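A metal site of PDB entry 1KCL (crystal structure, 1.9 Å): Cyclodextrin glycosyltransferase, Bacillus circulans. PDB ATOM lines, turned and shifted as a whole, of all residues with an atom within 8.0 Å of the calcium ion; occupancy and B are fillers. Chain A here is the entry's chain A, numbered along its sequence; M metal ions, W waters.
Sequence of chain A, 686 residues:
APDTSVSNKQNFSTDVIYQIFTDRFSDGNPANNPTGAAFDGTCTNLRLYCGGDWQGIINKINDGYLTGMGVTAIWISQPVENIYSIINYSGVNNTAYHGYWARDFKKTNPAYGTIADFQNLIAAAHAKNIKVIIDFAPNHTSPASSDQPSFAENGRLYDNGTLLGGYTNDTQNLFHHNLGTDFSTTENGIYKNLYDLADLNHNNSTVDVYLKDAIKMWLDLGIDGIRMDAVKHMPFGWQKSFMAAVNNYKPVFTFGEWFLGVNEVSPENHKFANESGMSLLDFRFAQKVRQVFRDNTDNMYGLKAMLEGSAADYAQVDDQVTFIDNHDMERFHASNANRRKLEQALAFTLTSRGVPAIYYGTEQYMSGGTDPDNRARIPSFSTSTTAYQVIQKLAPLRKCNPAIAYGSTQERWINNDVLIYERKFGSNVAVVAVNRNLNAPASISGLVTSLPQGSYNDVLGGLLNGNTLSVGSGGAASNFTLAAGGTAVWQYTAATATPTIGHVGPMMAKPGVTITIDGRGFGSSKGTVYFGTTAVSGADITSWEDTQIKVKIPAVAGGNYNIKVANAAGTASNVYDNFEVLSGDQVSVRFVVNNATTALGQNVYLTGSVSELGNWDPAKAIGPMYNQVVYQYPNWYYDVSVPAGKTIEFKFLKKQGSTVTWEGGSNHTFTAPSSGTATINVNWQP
The side-chain amide nitrogen (ND2) of Asn 33 sits close to the backbone carbonyl oxygen (O) of Pro 30 (3.0 Å).
N of Gly 28 is in hydrogen-bond range of OD1 of Asp 53.
The backbone NH (N) of Asp 53 sits at hydrogen-bond distance from the backbone carbonyl oxygen (O) of Ser 26 (3.1 Å).
OD1 of Asp 53 is in hydrogen-bond range of N of Gln 55 (3.3 Å).
The backbone NH (N) of Gly 56 lies within hydrogen-bond range of the side-chain carboxylate (OD1) of Asp 53 (2.8 Å).
OD1 of Asn 32 sits close to O of Ala 111 (3.2 Å).
The backbone NH of Ala 31 lies close to the side-chain amide oxygen of Asn 29, 3.1 Å away.
N of Gly 51 sits at hydrogen-bond distance from OD1 of Asp 23.
The calcium ion is bound by OD1 of Asn 33 (2.2 Å), OD1 of Asp 27 (2.3 Å), OD2 of Asp 53 (2.3 Å), OD1 of Asn 32 (2.4 Å), water W1 (2.5 Å), O of Asn 29 (2.5 Å) and O of Gly 51 (2.5 Å).
Within 4 Å of the calcium ion: Asp 27, Asn 29, Asn 32, Asn 33, Gly 51 and Asp 53.
The nearest printed residue that does not touch the calcium ion is Pro 30 (4.1 Å).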
ATOM      1  N   THR A  22      15.619  14.782  -2.422  1.00  0.00           N
ATOM      2  CA  THR A  22      14.786  13.929  -1.585  1.00  0.00           C
ATOM      3  C   THR A  22      14.124  14.596  -0.382  1.00  0.00           C
ATOM      4  O   THR A  22      12.920  14.474  -0.190  1.00  0.00           O
ATOM      5  CB  THR A  22      15.582  12.708  -1.101  1.00  0.00           C
ATOM      6  OG1 THR A  22      16.088  11.991  -2.229  1.00  0.00           O
ATOM      7  CG2 THR A  22      14.693  11.774  -0.279  1.00  0.00           C
ATOM      8  N   ASP A  23      14.904  15.317   0.414  1.00  0.00           N
ATOM      9  CA  ASP A  23      14.376  15.958   1.605  1.00  0.00           C
ATOM     10  C   ASP A  23      13.355  17.058   1.330  1.00  0.00           C
ATOM     11  O   ASP A  23      12.483  17.338   2.163  1.00  0.00           O
ATOM     12  CB  ASP A  23      15.517  16.553   2.429  1.00  0.00           C
ATOM     13  CG  ASP A  23      15.045  17.155   3.742  1.00  0.00           C
ATOM     14  OD1 ASP A  23      14.576  16.391   4.606  1.00  0.00           O
ATOM     15  OD2 ASP A  23      15.128  18.392   3.881  1.00  0.00           O
ATOM     16  N   SER A  26       8.860  15.206  -0.920  1.00  0.00           N
ATOM     17  CA  SER A  26       7.672  14.765  -0.196  1.00  0.00           C
ATOM     18  C   SER A  26       7.983  13.844   0.986  1.00  0.00           C
ATOM     19  O   SER A  26       8.633  12.805   0.824  1.00  0.00           O
ATOM     20  CB  SER A  26       6.713  14.051  -1.158  1.00  0.00           C
ATOM     21  OG  SER A  26       5.559  13.585  -0.476  1.00  0.00           O
ATOM     22  N   ASP A  27       7.510  14.231   2.158  1.00  0.00           N
ATOM     23  CA  ASP A  27       7.702  13.440   3.373  1.00  0.00           C
ATOM     24  C   ASP A  27       6.593  12.399   3.449  1.00  0.00           C
ATOM     25  O   ASP A  27       5.497  12.676   3.939  1.00  0.00           O
ATOM     26  CB  ASP A  27       7.661  14.356   4.607  1.00  0.00           C
ATOM     27  CG  ASP A  27       7.769  13.591   5.912  1.00  0.00           C
ATOM     28  OD1 ASP A  27       8.309  12.471   5.911  1.00  0.00           O
ATOM     29  OD2 ASP A  27       7.333  14.137   6.950  1.00  0.00           O
ATOM     30  N   GLY A  28       6.884  11.199   2.949  1.00  0.00           N
ATOM     31  CA  GLY A  28       5.904  10.131   2.935  1.00  0.00           C
ATOM     32  C   GLY A  28       5.888   9.292   4.204  1.00  0.00           C
ATOM     33  O   GLY A  28       4.977   8.492   4.410  1.00  0.00           O
ATOM     34  N   ASN A  29       6.891   9.474   5.055  1.00  0.00           N
ATOM     35  CA  ASN A  29       6.969   8.754   6.310  1.00  0.00           C
ATOM     36  C   ASN A  29       7.554   9.644   7.399  1.00  0.00           C
ATOM     37  O   ASN A  29       8.780   9.731   7.554  1.00  0.00           O
ATOM     38  CB  ASN A  29       7.813   7.487   6.145  1.00  0.00           C
ATOM     39  CG  ASN A  29       7.991   6.724   7.451  1.00  0.00           C
ATOM     40  OD1 ASN A  29       7.216   6.901   8.392  1.00  0.00           O
ATOM     41  ND2 ASN A  29       9.007   5.867   7.507  1.00  0.00           N
ATOM     42  N   PRO A  30       6.688  10.321   8.167  1.00  0.00           N
ATOM     43  CA  PRO A  30       7.099  11.218   9.254  1.00  0.00           C
ATOM     44  C   PRO A  30       7.888  10.518  10.358  1.00  0.00           C
ATOM     45  O   PRO A  30       8.620  11.158  11.104  1.00  0.00           O
ATOM     46  CB  PRO A  30       5.767  11.756   9.767  1.00  0.00           C
ATOM     47  CG  PRO A  30       4.890  11.707   8.549  1.00  0.00           C
ATOM     48  CD  PRO A  30       5.237  10.364   7.980  1.00  0.00           C
ATOM     49  N   ALA A  31       7.738   9.199  10.438  1.00  0.00           N
ATOM     50  CA  ALA A  31       8.402   8.404  11.470  1.00  0.00           C
ATOM     51  C   ALA A  31       9.918   8.422  11.390  1.00  0.00           C
ATOM     52  O   ALA A  31      10.598   8.311  12.406  1.00  0.00           O
ATOM     53  CB  ALA A  31       7.895   6.966  11.423  1.00  0.00           C
ATOM     54  N   ASN A  32      10.465   8.567  10.189  1.00  0.00           N
ATOM     55  CA  ASN A  32      11.918   8.584  10.030  1.00  0.00           C
ATOM     56  C   ASN A  32      12.487  10.002  10.022  1.00  0.00           C
ATOM     57  O   ASN A  32      13.685  10.194   9.794  1.00  0.00           O
ATOM     58  CB  ASN A  32      12.351   7.843   8.753  1.00  0.00           C
ATOM     59  CG  ASN A  32      11.748   8.444   7.489  1.00  0.00           C
ATOM     60  OD1 ASN A  32      11.552   9.658   7.397  1.00  0.00           O
ATOM     61  ND2 ASN A  32      11.485   7.595   6.504  1.00  0.00           N
ATOM     62  N   ASN A  33      11.635  10.994  10.273  1.00  0.00           N
ATOM     63  CA  ASN A  33      12.086  12.391  10.283  1.00  0.00           C
ATOM     64  C   ASN A  33      13.095  12.668  11.389  1.00  0.00           C
ATOM     65  O   ASN A  33      12.938  12.178  12.519  1.00  0.00           O
ATOM     66  CB  ASN A  33      10.897  13.350  10.472  1.00  0.00           C
ATOM     67  CG  ASN A  33       9.933  13.335   9.303  1.00  0.00           C
ATOM     68  OD1 ASN A  33      10.316  13.044   8.171  1.00  0.00           O
ATOM     69  ND2 ASN A  33       8.684  13.684   9.577  1.00  0.00           N
ATOM     70  N   PRO A  34      14.160  13.425  11.086  1.00  0.00           N
ATOM     71  CA  PRO A  34      15.134  13.745  12.120  1.00  0.00           C
ATOM     72  C   PRO A  34      14.411  14.553  13.201  1.00  0.00           C
ATOM     73  O   PRO A  34      13.305  15.027  12.969  1.00  0.00           O
ATOM     74  CB  PRO A  34      16.173  14.566  11.372  1.00  0.00           C
ATOM     75  CG  PRO A  34      16.145  13.952  10.008  1.00  0.00           C
ATOM     76  CD  PRO A  34      14.662  13.825   9.757  1.00  0.00           C
ATOM     77  N   PHE A  39      15.826  19.392  12.581  1.00  0.00           N
ATOM     78  CA  PHE A  39      14.572  19.275  11.832  1.00  0.00           C
ATOM     79  C   PHE A  39      13.685  20.513  11.876  1.00  0.00           C
ATOM     80  O   PHE A  39      13.647  21.245  12.863  1.00  0.00           O
ATOM     81  CB  PHE A  39      13.788  18.073  12.366  1.00  0.00           C
ATOM     82  CG  PHE A  39      12.502  17.818  11.645  1.00  0.00           C
ATOM     83  CD1 PHE A  39      12.498  17.301  10.352  1.00  0.00           C
ATOM     84  CD2 PHE A  39      11.275  18.092  12.260  1.00  0.00           C
ATOM     85  CE1 PHE A  39      11.304  17.053   9.682  1.00  0.00           C
ATOM     86  CE2 PHE A  39      10.079  17.854  11.589  1.00  0.00           C
ATOM     87  CZ  PHE A  39      10.091  17.329  10.297  1.00  0.00           C
ATOM     88  N   TYR A  49      16.744  19.494   8.113  1.00  0.00           N
ATOM     89  CA  TYR A  49      15.961  18.428   7.494  1.00  0.00           C
ATOM     90  C   TYR A  49      14.489  18.835   7.482  1.00  0.00           C
ATOM     91  O   TYR A  49      13.966  19.313   8.490  1.00  0.00           O
ATOM     92  CB  TYR A  49      16.127  17.122   8.272  1.00  0.00           C
ATOM     93  CG  TYR A  49      17.282  16.256   7.821  1.00  0.00           C
ATOM     94  CD1 TYR A  49      17.161  15.423   6.711  1.00  0.00           C
ATOM     95  CD2 TYR A  49      18.482  16.241   8.535  1.00  0.00           C
ATOM     96  CE1 TYR A  49      18.209  14.589   6.314  1.00  0.00           C
ATOM     97  CE2 TYR A  49      19.536  15.408   8.145  1.00  0.00           C
ATOM     98  CZ  TYR A  49      19.391  14.590   7.042  1.00  0.00           C
ATOM     99  OH  TYR A  49      20.417  13.752   6.666  1.00  0.00           O
ATOM    100  N   CYS A  50      13.833  18.634   6.347  1.00  0.00           N
ATOM    101  CA  CYS A  50      12.418  18.979   6.209  1.00  0.00           C
ATOM    102  C   CYS A  50      11.526  17.744   6.268  1.00  0.00           C
ATOM    103  O   CYS A  50      10.321  17.856   6.487  1.00  0.00           O
ATOM    104  CB  CYS A  50      12.210  19.746   4.901  1.00  0.00           C
ATOM    105  SG  CYS A  50      12.947  21.420   4.951  1.00  0.00           S
ATOM    106  N   GLY A  51      12.122  16.573   6.070  1.00  0.00           N
ATOM    107  CA  GLY A  51      11.358  15.342   6.159  1.00  0.00           C
ATOM    108  C   GLY A  51      11.146  14.551   4.878  1.00  0.00           C
ATOM    109  O   GLY A  51      10.651  13.422   4.930  1.00  0.00           O
ATOM    110  N   GLY A  52      11.518  15.122   3.737  1.00  0.00           N
ATOM    111  CA  GLY A  52      11.347  14.421   2.470  1.00  0.00           C
ATOM    112  C   GLY A  52      12.085  13.094   2.445  1.00  0.00           C
ATOM    113  O   GLY A  52      13.263  13.031   2.798  1.00  0.00           O
ATOM    114  N   ASP A  53      11.404  12.038   2.019  1.00  0.00           N
ATOM    115  CA  ASP A  53      11.999  10.705   1.991  1.00  0.00           C
ATOM    116  C   ASP A  53      11.633   9.886   0.750  1.00  0.00           C
ATOM    117  O   ASP A  53      10.920  10.357  -0.134  1.00  0.00           O
ATOM    118  CB  ASP A  53      11.599   9.926   3.239  1.00  0.00           C
ATOM    119  CG  ASP A  53      10.105  10.004   3.517  1.00  0.00           C
ATOM    120  OD1 ASP A  53       9.319   9.790   2.563  1.00  0.00           O
ATOM    121  OD2 ASP A  53       9.726  10.276   4.676  1.00  0.00           O
ATOM    122  N   TRP A  54      12.130   8.656   0.699  1.00  0.00           N
ATOM    123  CA  TRP A  54      11.870   7.766  -0.435  1.00  0.00           C
ATOM    124  C   TRP A  54      10.407   7.319  -0.508  1.00  0.00           C
ATOM    125  O   TRP A  54       9.887   7.082  -1.598  1.00  0.00           O
ATOM    126  CB  TRP A  54      12.802   6.546  -0.387  1.00  0.00           C
ATOM    127  CG  TRP A  54      14.263   6.900  -0.518  1.00  0.00           C
ATOM    128  CD1 TRP A  54      14.801   7.932  -1.234  1.00  0.00           C
ATOM    129  CD2 TRP A  54      15.371   6.195   0.062  1.00  0.00           C
ATOM    130  NE1 TRP A  54      16.170   7.914  -1.139  1.00  0.00           N
ATOM    131  CE2 TRP A  54      16.547   6.870  -0.345  1.00  0.00           C
ATOM    132  CE3 TRP A  54      15.488   5.073   0.895  1.00  0.00           C
ATOM    133  CZ2 TRP A  54      17.829   6.441   0.032  1.00  0.00           C
ATOM    134  CZ3 TRP A  54      16.762   4.652   1.278  1.00  0.00           C
ATOM    135  CH2 TRP A  54      17.915   5.333   0.851  1.00  0.00           C
ATOM    136  N   GLN A  55       9.748   7.203   0.641  1.00  0.00           N
ATOM    137  CA  GLN A  55       8.340   6.808   0.647  1.00  0.00           C
ATOM    138  C   GLN A  55       7.540   7.915  -0.050  1.00  0.00           C
ATOM    139  O   GLN A  55       6.544   7.643  -0.723  1.00  0.00           O
ATOM    140  CB  GLN A  55       7.826   6.619   2.074  1.00  0.00           C
ATOM    141  CG  GLN A  55       6.363   6.203   2.149  1.00  0.00           C
ATOM    142  CD  GLN A  55       6.091   4.876   1.456  1.00  0.00           C
ATOM    143  OE1 GLN A  55       6.637   3.842   1.850  1.00  0.00           O
ATOM    144  NE2 GLN A  55       5.248   4.896   0.430  1.00  0.00           N
ATOM    145  N   GLY A  56       7.990   9.150   0.131  1.00  0.00           N
ATOM    146  CA  GLY A  56       7.330  10.274  -0.506  1.00  0.00           C
ATOM    147  C   GLY A  56       7.485  10.192  -2.017  1.00  0.00           C
ATOM    148  O   GLY A  56       6.550  10.449  -2.762  1.00  0.00           O
ATOM    149  N   PRO A 110      19.077   7.065   7.138  1.00  0.00           N
ATOM    150  CA  PRO A 110      17.818   6.773   7.846  1.00  0.00           C
ATOM    151  C   PRO A 110      16.698   7.783   7.583  1.00  0.00           C
ATOM    152  O   PRO A 110      15.521   7.421   7.613  1.00  0.00           O
ATOM    153  CB  PRO A 110      18.256   6.763   9.310  1.00  0.00           C
ATOM    154  CG  PRO A 110      19.667   6.263   9.230  1.00  0.00           C
ATOM    155  CD  PRO A 110      20.216   7.050   8.063  1.00  0.00           C
ATOM    156  N   ALA A 111      17.064   9.040   7.352  1.00  0.00           N
ATOM    157  CA  ALA A 111      16.074  10.084   7.084  1.00  0.00           C
ATOM    158  C   ALA A 111      15.331   9.825   5.778  1.00  0.00           C
ATOM    159  O   ALA A 111      14.146  10.132   5.665  1.00  0.00           O
ATOM    160  CB  ALA A 111      16.756  11.443   7.049  1.00  0.00           C
ATOM    161  N   TYR A 112      16.024   9.247   4.795  1.00  0.00           N
ATOM    162  CA  TYR A 112      15.405   8.940   3.519  1.00  0.00           C
ATOM    163  C   TYR A 112      14.659   7.611   3.624  1.00  0.00           C
ATOM    164  O   TYR A 112      13.549   7.471   3.117  1.00  0.00           O
ATOM    165  CB  TYR A 112      16.444   8.832   2.399  1.00  0.00           C
ATOM    166  CG  TYR A 112      17.271  10.084   2.161  1.00  0.00           C
ATOM    167  CD1 TYR A 112      16.814  11.343   2.531  1.00  0.00           C
ATOM    168  CD2 TYR A 112      18.521   9.998   1.532  1.00  0.00           C
ATOM    169  CE1 TYR A 112      17.567  12.490   2.286  1.00  0.00           C
ATOM    170  CE2 TYR A 112      19.283  11.136   1.280  1.00  0.00           C
ATOM    171  CZ  TYR A 112      18.800  12.380   1.664  1.00  0.00           C
ATOM    172  OH  TYR A 112      19.559  13.497   1.405  1.00  0.00           O
ATOM    173  N   GLY A 113      15.284   6.633   4.281  1.00  0.00           N
ATOM    174  CA  GLY A 113      14.660   5.337   4.444  1.00  0.00           C
ATOM    175  C   GLY A 113      15.637   4.209   4.698  1.00  0.00           C
ATOM    176  O   GLY A 113      16.845   4.436   4.803  1.00  0.00           O
HETATM  177 CA    CA M   1      10.247  11.515   6.541  1.00  0.00          CA
HETATM  178  O   HOH W   1      12.648  12.015   6.701  1.00  0.00           O
